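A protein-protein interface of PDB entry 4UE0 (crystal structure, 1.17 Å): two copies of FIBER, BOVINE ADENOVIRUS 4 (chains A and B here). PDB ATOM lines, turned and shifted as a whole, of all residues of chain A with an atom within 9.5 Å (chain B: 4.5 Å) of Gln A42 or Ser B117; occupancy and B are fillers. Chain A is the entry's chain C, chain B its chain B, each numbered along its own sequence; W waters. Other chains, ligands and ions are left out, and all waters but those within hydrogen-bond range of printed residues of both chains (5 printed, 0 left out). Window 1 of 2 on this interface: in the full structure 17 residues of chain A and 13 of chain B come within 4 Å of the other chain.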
ATOM      1  N   VAL A  13       9.057  18.530  -3.211  1.00  0.00           N
ATOM      2  CA  VAL A  13       8.391  17.260  -3.470  1.00  0.00           C
ATOM      3  C   VAL A  13       9.267  16.492  -4.440  1.00  0.00           C
ATOM      4  O   VAL A  13       9.583  16.984  -5.526  1.00  0.00           O
ATOM      5  CB  VAL A  13       6.948  17.448  -3.944  1.00  0.00           C
ATOM      6  CG1 VAL A  13       6.269  16.122  -4.169  1.00  0.00           C
ATOM      7  CG2 VAL A  13       6.177  18.227  -2.896  1.00  0.00           C
ATOM      8  N   PHE A  19       8.073   6.473  -6.331  1.00  0.00           N
ATOM      9  CA  PHE A  19       7.264   7.016  -5.246  1.00  0.00           C
ATOM     10  C   PHE A  19       7.642   8.451  -4.957  1.00  0.00           C
ATOM     11  O   PHE A  19       8.601   8.965  -5.513  1.00  0.00           O
ATOM     12  CB  PHE A  19       7.282   6.112  -3.994  1.00  0.00           C
ATOM     13  CG  PHE A  19       8.620   6.000  -3.325  1.00  0.00           C
ATOM     14  CD1 PHE A  19       9.546   5.052  -3.743  1.00  0.00           C
ATOM     15  CD2 PHE A  19       8.950   6.828  -2.261  1.00  0.00           C
ATOM     16  CE1 PHE A  19      10.777   4.932  -3.113  1.00  0.00           C
ATOM     17  CE2 PHE A  19      10.178   6.708  -1.640  1.00  0.00           C
ATOM     18  CZ  PHE A  19      11.086   5.768  -2.066  1.00  0.00           C
ATOM     19  N   ILE A  20       6.814   9.091  -4.129  1.00  0.00           N
ATOM     20  CA  ILE A  20       6.938  10.512  -3.792  1.00  0.00           C
ATOM     21  C   ILE A  20       7.284  10.646  -2.314  1.00  0.00           C
ATOM     22  O   ILE A  20       6.670   9.989  -1.466  1.00  0.00           O
ATOM     23  CB  ILE A  20       5.577  11.258  -4.048  1.00  0.00           C
ATOM     24  CG1 ILE A  20       5.217  11.194  -5.526  1.00  0.00           C
ATOM     25  CG2 ILE A  20       5.574  12.679  -3.496  1.00  0.00           C
ATOM     26  CD1 ILE A  20       6.069  12.083  -6.376  1.00  0.00           C
ATOM     27  N   ILE A  21       8.230  11.541  -2.021  1.00  0.00           N
ATOM     28  CA  ILE A  21       8.431  12.025  -0.653  1.00  0.00           C
ATOM     29  C   ILE A  21       8.369  13.540  -0.687  1.00  0.00           C
ATOM     30  O   ILE A  21       8.780  14.156  -1.652  1.00  0.00           O
ATOM     31  CB  ILE A  21       9.774  11.390  -0.171  1.00  0.00           C
ATOM     32  CG1 ILE A  21      10.075  11.619   1.307  1.00  0.00           C
ATOM     33  CG2 ILE A  21      10.951  11.851  -1.025  1.00  0.00           C
ATOM     34  CD1 ILE A  21      11.270  10.806   1.795  1.00  0.00           C
ATOM     35  N   ALA A  22       7.797  14.123   0.348  1.00  0.00           N
ATOM     36  CA  ALA A  22       7.502  15.556   0.409  1.00  0.00           C
ATOM     37  C   ALA A  22       8.125  16.145   1.651  1.00  0.00           C
ATOM     38  O   ALA A  22       7.783  15.771   2.777  1.00  0.00           O
ATOM     39  CB  ALA A  22       6.005  15.777   0.377  1.00  0.00           C
ATOM     40  N   LEU A  23       9.036  17.075   1.414  1.00  0.00           N
ATOM     41  CA  LEU A  23       9.851  17.698   2.453  1.00  0.00           C
ATOM     42  C   LEU A  23       9.562  19.175   2.583  1.00  0.00           C
ATOM     43  O   LEU A  23       9.213  19.854   1.618  1.00  0.00           O
ATOM     44  CB  LEU A  23      11.321  17.588   2.101  1.00  0.00           C
ATOM     45  CG  LEU A  23      11.864  16.205   1.824  1.00  0.00           C
ATOM     46  CD1 LEU A  23      13.218  16.287   1.130  1.00  0.00           C
ATOM     47  CD2 LEU A  23      12.021  15.511   3.132  1.00  0.00           C
ATOM     48  N   GLY A  24       9.781  19.681   3.793  1.00  0.00           N
ATOM     49  CA  GLY A  24       9.752  21.092   4.081  1.00  0.00           C
ATOM     50  C   GLY A  24      10.940  21.520   4.883  1.00  0.00           C
ATOM     51  O   GLY A  24      11.476  20.741   5.674  1.00  0.00           O
ATOM     52  N   ASN A  39      11.461  18.707   7.655  1.00  0.00           N
ATOM     53  CA  ASN A  39      10.470  17.708   7.931  1.00  0.00           C
ATOM     54  C   ASN A  39      10.008  17.027   6.682  1.00  0.00           C
ATOM     55  O   ASN A  39      10.277  17.449   5.558  1.00  0.00           O
ATOM     56  CB  ASN A  39       9.314  18.317   8.681  1.00  0.00           C
ATOM     57  CG  ASN A  39       8.716  19.464   7.935  1.00  0.00           C
ATOM     58  OD1 ASN A  39       8.509  19.367   6.738  1.00  0.00           O
ATOM     59  ND2 ASN A  39       8.466  20.574   8.618  1.00  0.00           N
ATOM     60  N   CYS A  40       9.295  15.950   6.908  1.00  0.00           N
ATOM     61  CA  CYS A  40       8.930  15.032   5.827  1.00  0.00           C
ATOM     62  C   CYS A  40       7.563  14.453   6.161  1.00  0.00           C
ATOM     63  O   CYS A  40       7.347  13.981   7.278  1.00  0.00           O
ATOM     64  CB  CYS A  40       9.956  13.910   5.772  1.00  0.00           C
ATOM     65  SG  CYS A  40       9.800  12.807   4.380  1.00  0.00           S
ATOM     66  N   SER A  41       6.633  14.493   5.214  1.00  0.00           N
ATOM     67  CA  SER A  41       5.341  13.848   5.410  1.00  0.00           C
ATOM     68  C   SER A  41       5.483  12.317   5.339  1.00  0.00           C
ATOM     69  O   SER A  41       6.494  11.782   4.870  1.00  0.00           O
ATOM     70  CB  SER A  41       4.337  14.312   4.360  1.00  0.00           C
ATOM     71  OG  SER A  41       4.005  15.682   4.559  1.00  0.00           O
ATOM     72  N   GLN A  42       4.437  11.629   5.779  1.00  0.00           N
ATOM     73  CA  GLN A  42       4.427  10.189   5.604  1.00  0.00           C
ATOM     74  C   GLN A  42       4.594   9.838   4.119  1.00  0.00           C
ATOM     75  O   GLN A  42       4.164  10.590   3.230  1.00  0.00           O
ATOM     76  CB  GLN A  42       3.151   9.548   6.162  1.00  0.00           C
ATOM     77  CG  GLN A  42       1.861   9.982   5.474  1.00  0.00           C
ATOM     78  CD  GLN A  42       0.664   9.433   6.213  1.00  0.00           C
ATOM     79  OE1 GLN A  42       0.499   9.696   7.401  1.00  0.00           O
ATOM     80  NE2 GLN A  42      -0.174   8.686   5.518  1.00  0.00           N
ATOM     81  N   PHE A  43       5.180   8.666   3.852  1.00  0.00           N
ATOM     82  CA  PHE A  43       5.380   8.218   2.472  1.00  0.00           C
ATOM     83  C   PHE A  43       5.416   6.714   2.438  1.00  0.00           C
ATOM     84  O   PHE A  43       5.647   6.065   3.452  1.00  0.00           O
ATOM     85  CB  PHE A  43       6.655   8.796   1.848  1.00  0.00           C
ATOM     86  CG  PHE A  43       7.928   8.303   2.475  1.00  0.00           C
ATOM     87  CD1 PHE A  43       8.403   8.865   3.655  1.00  0.00           C
ATOM     88  CD2 PHE A  43       8.670   7.291   1.871  1.00  0.00           C
ATOM     89  CE1 PHE A  43       9.575   8.392   4.268  1.00  0.00           C
ATOM     90  CE2 PHE A  43       9.827   6.808   2.465  1.00  0.00           C
ATOM     91  CZ  PHE A  43      10.274   7.366   3.657  1.00  0.00           C
ATOM     92  N   MET A  44       5.205   6.158   1.247  1.00  0.00           N
ATOM     93  CA  MET A  44       5.183   4.700   1.083  1.00  0.00           C
ATOM     94  C   MET A  44       6.245   4.280   0.075  1.00  0.00           C
ATOM     95  O   MET A  44       6.042   4.406  -1.145  1.00  0.00           O
ATOM     96  CB  MET A  44       3.804   4.208   0.665  1.00  0.00           C
ATOM     97  CG  MET A  44       3.746   2.690   0.577  1.00  0.00           C
ATOM     98  SD  MET A  44       2.176   1.996   0.145  1.00  0.00           S
ATOM     99  CE  MET A  44       1.322   2.223   1.722  1.00  0.00           C
ATOM    100  N   PRO A  45       7.398   3.783   0.557  1.00  0.00           N
ATOM    101  CA  PRO A  45       8.383   3.306  -0.398  1.00  0.00           C
ATOM    102  C   PRO A  45       7.875   2.032  -1.063  1.00  0.00           C
ATOM    103  O   PRO A  45       7.087   1.300  -0.496  1.00  0.00           O
ATOM    104  CB  PRO A  45       9.587   2.984   0.483  1.00  0.00           C
ATOM    105  CG  PRO A  45       9.010   2.622   1.795  1.00  0.00           C
ATOM    106  CD  PRO A  45       7.790   3.495   1.956  1.00  0.00           C
ATOM    107  N   CYS A  74      11.938   7.503  12.351  1.00  0.00           N
ATOM    108  CA  CYS A  74      10.613   7.226  11.799  1.00  0.00           C
ATOM    109  C   CYS A  74      10.277   5.771  12.042  1.00  0.00           C
ATOM    110  O   CYS A  74      11.122   5.015  12.521  1.00  0.00           O
ATOM    111  CB  CYS A  74      10.541   7.632  10.314  1.00  0.00           C
ATOM    112  SG  CYS A  74      11.553   6.618   9.252  1.00  0.00           S
ATOM    113  N   THR A  75       9.054   5.372  11.719  1.00  0.00           N
ATOM    114  CA  THR A  75       8.617   4.002  11.948  1.00  0.00           C
ATOM    115  C   THR A  75       7.849   3.471  10.755  1.00  0.00           C
ATOM    116  O   THR A  75       7.293   4.211   9.943  1.00  0.00           O
ATOM    117  CB  THR A  75       7.720   3.862  13.207  1.00  0.00           C
ATOM    118  OG1 THR A  75       6.433   4.468  12.994  1.00  0.00           O
ATOM    119  CG2 THR A  75       8.382   4.412  14.441  1.00  0.00           C
ATOM    120  N   GLN A  76       7.770   2.143  10.723  1.00  0.00           N
ATOM    121  CA  GLN A  76       6.781   1.407   9.929  1.00  0.00           C
ATOM    122  C   GLN A  76       6.100   0.376  10.842  1.00  0.00           C
ATOM    123  O   GLN A  76       6.736  -0.193  11.716  1.00  0.00           O
ATOM    124  CB  GLN A  76       7.386   0.672   8.747  1.00  0.00           C
ATOM    125  CG  GLN A  76       7.911   1.581   7.658  1.00  0.00           C
ATOM    126  CD  GLN A  76       8.525   0.778   6.544  1.00  0.00           C
ATOM    127  OE1 GLN A  76       9.480   0.039   6.765  1.00  0.00           O
ATOM    128  NE2 GLN A  76       8.009   0.934   5.333  1.00  0.00           N
ATOM    129  N   ILE A 109       4.655  -0.329   2.802  1.00  0.00           N
ATOM    130  CA  ILE A 109       4.153  -0.016   4.124  1.00  0.00           C
ATOM    131  C   ILE A 109       4.458   1.467   4.393  1.00  0.00           C
ATOM    132  O   ILE A 109       5.571   1.939   4.130  1.00  0.00           O
ATOM    133  CB  ILE A 109       4.775  -0.923   5.204  1.00  0.00           C
ATOM    134  CG1 ILE A 109       4.381  -2.392   4.960  1.00  0.00           C
ATOM    135  CG2 ILE A 109       4.366  -0.466   6.598  1.00  0.00           C
ATOM    136  CD1 ILE A 109       4.909  -3.345   6.007  1.00  0.00           C
ATOM    137  N   MET A 110       3.466   2.191   4.899  1.00  0.00           N
ATOM    138  CA  MET A 110       3.635   3.606   5.179  1.00  0.00           C
ATOM    139  C   MET A 110       4.732   3.849   6.222  1.00  0.00           C
ATOM    140  O   MET A 110       4.823   3.133   7.223  1.00  0.00           O
ATOM    141  CB  MET A 110       2.327   4.215   5.667  1.00  0.00           C
ATOM    142  CG  MET A 110       2.284   5.730   5.570  1.00  0.00           C
ATOM    143  SD  MET A 110       2.212   6.360   3.881  1.00  0.00           S
ATOM    144  CE  MET A 110       0.575   5.851   3.422  1.00  0.00           C
ATOM    145  N   VAL A 111       5.535   4.876   5.978  1.00  0.00           N
ATOM    146  CA  VAL A 111       6.514   5.403   6.913  1.00  0.00           C
ATOM    147  C   VAL A 111       5.960   6.667   7.562  1.00  0.00           C
ATOM    148  O   VAL A 111       5.418   7.516   6.870  1.00  0.00           O
ATOM    149  CB  VAL A 111       7.841   5.714   6.176  1.00  0.00           C
ATOM    150  CG1 VAL A 111       8.850   6.282   7.151  1.00  0.00           C
ATOM    151  CG2 VAL A 111       8.389   4.504   5.430  1.00  0.00           C
ATOM    152  N   SER A 112       6.097   6.770   8.888  1.00  0.00           N
ATOM    153  CA  SER A 112       5.575   7.922   9.593  1.00  0.00           C
ATOM    154  C   SER A 112       6.341   9.206   9.227  1.00  0.00           C
ATOM    155  O   SER A 112       7.513   9.187   8.920  1.00  0.00           O
ATOM    156  CB  SER A 112       5.591   7.671  11.109  1.00  0.00           C
ATOM    157  OG  SER A 112       6.859   7.259  11.573  1.00  0.00           O
ATOM    158  N   ALA A 113       5.622  10.312   9.295  1.00  0.00           N
ATOM    159  CA  ALA A 113       6.209  11.637   9.134  1.00  0.00           C
ATOM    160  C   ALA A 113       7.254  11.884  10.215  1.00  0.00           C
ATOM    161  O   ALA A 113       7.140  11.345  11.316  1.00  0.00           O
ATOM    162  CB  ALA A 113       5.143  12.702   9.239  1.00  0.00           C
ATOM    163  N   TRP A 114       8.237  12.723   9.905  1.00  0.00           N
ATOM    164  CA  TRP A 114       9.301  13.023  10.843  1.00  0.00           C
ATOM    165  C   TRP A 114       9.759  14.448  10.694  1.00  0.00           C
ATOM    166  O   TRP A 114       9.556  15.081   9.667  1.00  0.00           O
ATOM    167  CB  TRP A 114      10.466  12.023  10.719  1.00  0.00           C
ATOM    168  CG  TRP A 114      11.034  11.906   9.337  1.00  0.00           C
ATOM    169  CD1 TRP A 114      10.712  10.951   8.413  1.00  0.00           C
ATOM    170  CD2 TRP A 114      12.046  12.749   8.719  1.00  0.00           C
ATOM    171  NE1 TRP A 114      11.447  11.132   7.275  1.00  0.00           N
ATOM    172  CE2 TRP A 114      12.246  12.240   7.416  1.00  0.00           C
ATOM    173  CE3 TRP A 114      12.738  13.896   9.113  1.00  0.00           C
ATOM    174  CZ2 TRP A 114      13.110  12.822   6.519  1.00  0.00           C
ATOM    175  CZ3 TRP A 114      13.593  14.515   8.195  1.00  0.00           C
ATOM    176  CH2 TRP A 114      13.785  13.960   6.920  1.00  0.00           C
ATOM    177  N   THR A 115      10.396  14.922  11.762  1.00  0.00           N
ATOM    178  CA  THR A 115      10.963  16.255  11.801  1.00  0.00           C
ATOM    179  C   THR A 115      12.309  16.239  12.460  1.00  0.00           C
ATOM    180  O   THR A 115      12.467  15.659  13.522  1.00  0.00           O
ATOM    181  CB  THR A 115      10.068  17.276  12.538  1.00  0.00           C
ATOM    182  OG1 THR A 115       8.785  17.330  11.953  1.00  0.00           O
ATOM    183  CG2 THR A 115      10.612  18.670  12.402  1.00  0.00           C
ATOM    184  N   ARG B  33       3.440  22.018  -1.871  1.00  0.00           N
ATOM    185  CA  ARG B  33       3.320  20.952  -0.872  1.00  0.00           C
ATOM    186  C   ARG B  33       2.116  21.233   0.024  1.00  0.00           C
ATOM    187  O   ARG B  33       2.205  21.924   1.033  1.00  0.00           O
ATOM    188  CB  ARG B  33       4.607  20.915  -0.062  1.00  0.00           C
ATOM    189  CG  ARG B  33       4.623  19.755   0.904  1.00  0.00           C
ATOM    190  CD  ARG B  33       5.679  19.888   1.946  1.00  0.00           C
ATOM    191  NE  ARG B  33       5.570  18.809   2.928  1.00  0.00           N
ATOM    192  CZ  ARG B  33       6.078  18.853   4.157  1.00  0.00           C
ATOM    193  NH1 ARG B  33       6.650  19.932   4.641  1.00  0.00           N
ATOM    194  NH2 ARG B  33       5.955  17.806   4.923  1.00  0.00           N
ATOM    195  N   ILE B  35      -0.464  20.429   2.600  1.00  0.00           N
ATOM    196  CA  ILE B  35      -0.308  19.561   3.757  1.00  0.00           C
ATOM    197  C   ILE B  35      -1.588  19.481   4.595  1.00  0.00           C
ATOM    198  O   ILE B  35      -2.270  20.462   4.834  1.00  0.00           O
ATOM    199  CB  ILE B  35       0.846  20.038   4.677  1.00  0.00           C
ATOM    200  CG1 ILE B  35       2.127  20.296   3.922  1.00  0.00           C
ATOM    201  CG2 ILE B  35       1.157  18.951   5.693  1.00  0.00           C
ATOM    202  CD1 ILE B  35       3.222  20.932   4.703  1.00  0.00           C
ATOM    203  N   TYR B  36      -1.824  18.270   5.108  1.00  0.00           N
ATOM    204  CA  TYR B  36      -2.857  17.985   6.106  1.00  0.00           C
ATOM    205  C   TYR B  36      -2.152  17.442   7.347  1.00  0.00           C
ATOM    206  O   TYR B  36      -1.401  16.479   7.246  1.00  0.00           O
ATOM    207  CB  TYR B  36      -3.825  16.933   5.575  1.00  0.00           C
ATOM    208  CG  TYR B  36      -4.535  17.380   4.328  1.00  0.00           C
ATOM    209  CD1 TYR B  36      -3.981  17.172   3.092  1.00  0.00           C
ATOM    210  CD2 TYR B  36      -5.722  18.081   4.393  1.00  0.00           C
ATOM    211  CE1 TYR B  36      -4.601  17.630   1.934  1.00  0.00           C
ATOM    212  CE2 TYR B  36      -6.363  18.536   3.250  1.00  0.00           C
ATOM    213  CZ  TYR B  36      -5.794  18.289   2.020  1.00  0.00           C
ATOM    214  OH  TYR B  36      -6.416  18.711   0.868  1.00  0.00           O
ATOM    215  N   SER B  68      -5.494   7.041   1.840  1.00  0.00           N
ATOM    216  CA  SER B  68      -4.561   6.564   2.862  1.00  0.00           C
ATOM    217  C   SER B  68      -4.855   7.182   4.246  1.00  0.00           C
ATOM    218  O   SER B  68      -4.966   8.404   4.386  1.00  0.00           O
ATOM    219  CB  SER B  68      -3.104   6.869   2.482  1.00  0.00           C
ATOM    220  OG  SER B  68      -2.747   8.214   2.782  1.00  0.00           O
ATOM    221  N   PRO B  69      -4.925   6.335   5.277  1.00  0.00           N
ATOM    222  CA  PRO B  69      -5.017   6.888   6.617  1.00  0.00           C
ATOM    223  C   PRO B  69      -3.746   7.631   7.041  1.00  0.00           C
ATOM    224  O   PRO B  69      -2.656   7.384   6.486  1.00  0.00           O
ATOM    225  CB  PRO B  69      -5.232   5.664   7.506  1.00  0.00           C
ATOM    226  CG  PRO B  69      -4.771   4.519   6.725  1.00  0.00           C
ATOM    227  CD  PRO B  69      -4.840   4.863   5.276  1.00  0.00           C
ATOM    228  N   PHE B  70      -3.885   8.511   8.023  1.00  0.00           N
ATOM    229  CA  PHE B  70      -2.709   9.067   8.681  1.00  0.00           C
ATOM    230  C   PHE B  70      -2.002   7.965   9.463  1.00  0.00           C
ATOM    231  O   PHE B  70      -2.649   7.115  10.084  1.00  0.00           O
ATOM    232  CB  PHE B  70      -3.111  10.172   9.628  1.00  0.00           C
ATOM    233  CG  PHE B  70      -3.667  11.385   8.963  1.00  0.00           C
ATOM    234  CD1 PHE B  70      -2.835  12.412   8.568  1.00  0.00           C
ATOM    235  CD2 PHE B  70      -5.041  11.522   8.758  1.00  0.00           C
ATOM    236  CE1 PHE B  70      -3.348  13.556   7.980  1.00  0.00           C
ATOM    237  CE2 PHE B  70      -5.561  12.662   8.144  1.00  0.00           C
ATOM    238  CZ  PHE B  70      -4.706  13.680   7.770  1.00  0.00           C
ATOM    239  N   TYR B  71      -0.659   8.010   9.448  1.00  0.00           N
ATOM    240  CA  TYR B  71       0.169   7.079  10.199  1.00  0.00           C
ATOM    241  C   TYR B  71       1.227   7.832  10.969  1.00  0.00           C
ATOM    242  O   TYR B  71       2.047   8.534  10.374  1.00  0.00           O
ATOM    243  CB  TYR B  71       0.802   5.999   9.265  1.00  0.00           C
ATOM    244  CG  TYR B  71       1.700   5.081  10.066  1.00  0.00           C
ATOM    245  CD1 TYR B  71       1.175   4.151  10.967  1.00  0.00           C
ATOM    246  CD2 TYR B  71       3.056   5.210   9.990  1.00  0.00           C
ATOM    247  CE1 TYR B  71       1.997   3.424  11.791  1.00  0.00           C
ATOM    248  CE2 TYR B  71       3.884   4.462  10.804  1.00  0.00           C
ATOM    249  CZ  TYR B  71       3.368   3.587  11.722  1.00  0.00           C
ATOM    250  OH  TYR B  71       4.158   2.877  12.618  1.00  0.00           O
ATOM    251  N   THR B 115       2.340  13.564  15.959  1.00  0.00           N
ATOM    252  CA  THR B 115       1.901  14.365  14.819  1.00  0.00           C
ATOM    253  C   THR B 115       2.001  13.513  13.565  1.00  0.00           C
ATOM    254  O   THR B 115       2.982  12.828  13.323  1.00  0.00           O
ATOM    255  CB  THR B 115       2.757  15.633  14.621  1.00  0.00           C
ATOM    256  OG1 THR B 115       2.695  16.487  15.746  1.00  0.00           O
ATOM    257  CG2 THR B 115       2.266  16.445  13.491  1.00  0.00           C
ATOM    258  N   ALA B 116       0.964  13.598  12.752  1.00  0.00           N
ATOM    259  CA  ALA B 116       0.889  12.966  11.437  1.00  0.00           C
ATOM    260  C   ALA B 116       0.787  14.077  10.387  1.00  0.00           C
ATOM    261  O   ALA B 116       0.156  15.102  10.625  1.00  0.00           O
ATOM    262  CB  ALA B 116      -0.329  12.045  11.347  1.00  0.00           C
ATOM    263  N   SER B 117       1.408  13.831   9.241  1.00  0.00           N
ATOM    264  CA  SER B 117       1.448  14.793   8.162  1.00  0.00           C
ATOM    265  C   SER B 117       1.297  14.049   6.844  1.00  0.00           C
ATOM    266  O   SER B 117       2.109  13.171   6.539  1.00  0.00           O
ATOM    267  CB  SER B 117       2.836  15.498   8.168  1.00  0.00           C
ATOM    268  OG  SER B 117       2.979  16.342   7.033  1.00  0.00           O
ATOM    269  N   ILE B 118       0.314  14.468   6.032  1.00  0.00           N
ATOM    270  CA  ILE B 118       0.134  13.988   4.661  1.00  0.00           C
ATOM    271  C   ILE B 118       0.300  15.160   3.719  1.00  0.00           C
ATOM    272  O   ILE B 118      -0.279  16.206   3.930  1.00  0.00           O
ATOM    273  CB  ILE B 118      -1.273  13.378   4.498  1.00  0.00           C
ATOM    274  CG1 ILE B 118      -1.350  12.023   5.185  1.00  0.00           C
ATOM    275  CG2 ILE B 118      -1.644  13.248   3.025  1.00  0.00           C
ATOM    276  CD1 ILE B 118      -2.711  11.368   5.195  1.00  0.00           C
ATOM    277  N   THR B 119       1.087  14.955   2.672  1.00  0.00           N
ATOM    278  CA  THR B 119       1.136  15.900   1.558  1.00  0.00           C
ATOM    279  C   THR B 119       0.279  15.352   0.452  1.00  0.00           C
ATOM    280  O   THR B 119       0.453  14.214   0.026  1.00  0.00           O
ATOM    281  CB  THR B 119       2.563  16.140   1.085  1.00  0.00           C
ATOM    282  OG1 THR B 119       3.281  16.818   2.101  1.00  0.00           O
ATOM    283  CG2 THR B 119       2.582  16.968  -0.159  1.00  0.00           C
HETATM  284  O   HOH W   1       2.199  11.016   9.140  1.00  0.00           O
HETATM  285  O   HOH W   2       4.512  10.850  12.270  1.00  0.00           O
HETATM  286  O   HOH W   3       6.111  13.806  13.231  1.00  0.00           O
HETATM  287  O   HOH W   4       2.118  12.225   2.450  1.00  0.00           O
HETATM  288  O   HOH W   5      -0.035   9.388   2.444  1.00  0.00           O
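Hydrophobic or aromatic side chains of chain A that line the printed part of chain B: Ala A22, Met A110 and Ala A113.
Hydrophobic or aromatic side chains of chain B that line the printed part of chain A: Tyr B71 and Ile B118.
Among the printed residues, no Asp or Glu carboxylate lies within 4 Å of a Lys or Arg side-chain nitrogen of the other chain.
Among the printed residues, pairs that only touch across the chains: Ala A22 with Thr B119, Gln A42 with Ile B118, Gln A42 with Phe B70, Leu A23 with Arg B33, Ser A112 with Tyr B71, Gln A76 with Tyr B71, Ala A113 with Ser B117, Gln A42 with Ser B68, Ser A41 with Ile B118, Met A110 with Tyr B71, Cys A40 with Arg B33 and Met A110 with Ser B68.
The guanidinium group of Arg B33 is in hydrogen-bond range of the backbone carbonyl oxygen of Ala A22 (3.5 Å).
The side-chain amide oxygen (OD1) of Asn A39 is in hydrogen-bond range of the guanidinium group (NH1) of Arg B33 (2.9 Å).
The side-chain hydroxyl of Ser A41 lies within hydrogen-bond range of the guanidinium group of Arg B33 (2.9 Å).
O of Pro B69 sits at hydrogen-bond distance from NE2 of Gln A42.
The side-chain amide oxygen of Gln A42 sits at hydrogen-bond distance from the backbone NH of Tyr B71 (2.9 Å).
The side-chain hydroxyl (OG1) of Thr A75 sits at hydrogen-bond distance from the side-chain hydroxyl (OH) of Tyr B71 (2.8 Å).
OG of Ser B117 is in hydrogen-bond range of OG of Ser A41 (2.8 Å).
The backbone carbonyl oxygen (O) of Ser B117 lies within hydrogen-bond range of the backbone NH (N) of Gln A42 (2.9 Å).
OG of Ser A41 lies within hydrogen-bond range of OG1 of Thr B119 (2.8 Å).
The backbone NH (N) of Gly A24 lies close to the guanidinium group (NH1) of Arg B33 (3.3 Å).
The guanidinium group of Arg B33 is in hydrogen-bond range of the side-chain hydroxyl of Thr B119 (3.1 Å).
The backbone carbonyl oxygen (O) of Ile B118 sits at hydrogen-bond distance from the backbone NH (N) of Tyr B36, 2.8 Å away.
O of Ala A22 lies within hydrogen-bond range of N of Ser A41, at 3.0 Å.
The side-chain sulfur (SD) of Met A110 lies close to the side-chain amide nitrogen (NE2) of Gln A42 (3.7 Å).
N of Phe A43 lies close to SD of Met A110 (3.8 Å).
The backbone carbonyl oxygen of Ile A109 is in hydrogen-bond range of the side-chain amide nitrogen of Gln A76 (2.9 Å).
Position printed for both chains: 115.
Of the printed residues of chain B, Cys A40 touches Arg B33.
Printed residues of chain B within 4 Å of Gln A42: Ser B68, Pro B69, Phe B70, Tyr B71, Ser B117 and Ile B118.
Tyr B36 touches none of the printed residues of chain A.
Of the printed residues of chain A, Phe B70 touches Gln A42 (3.5 Å).
Ser B117 touches just these residues of chain A: Ser A41 (2.8 Å), Gln A42 (2.9 Å) and Ala A113 (3.8 Å).
Of chain A, only Ser A41 and Gln A42 come within 4 Å of Ile B118.
The nearest printed residue of chain B that does not touch Gln A42 is Ala B116 (4.7 Å).
The nearest printed residue of chain A that does not touch Ser B117 is Cys A40 (4.8 Å).
The nearest printed residue of chain A that does not touch Arg B33 is Val A13 (4.2 Å).
Water W2 bridges O of Thr B115 (2.7 Å) and O of Ala A113 (2.8 Å).
Water W4 bridges the backbone carbonyl oxygen of Gln A42 (2.7 Å) and the backbone NH of Thr B119 (2.9 Å).
Water W1 lies within hydrogen-bond range of OE1 of Gln A42, O of Tyr B71, N of Ser B117 and N of Ala A113.
Water W5 bridges OG of Ser B68 and NE2 of Gln A42.
Water W3 lies within hydrogen-bond range of O of Thr B115 (3.3 Å) and O of Ala A113 (3.3 Å).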
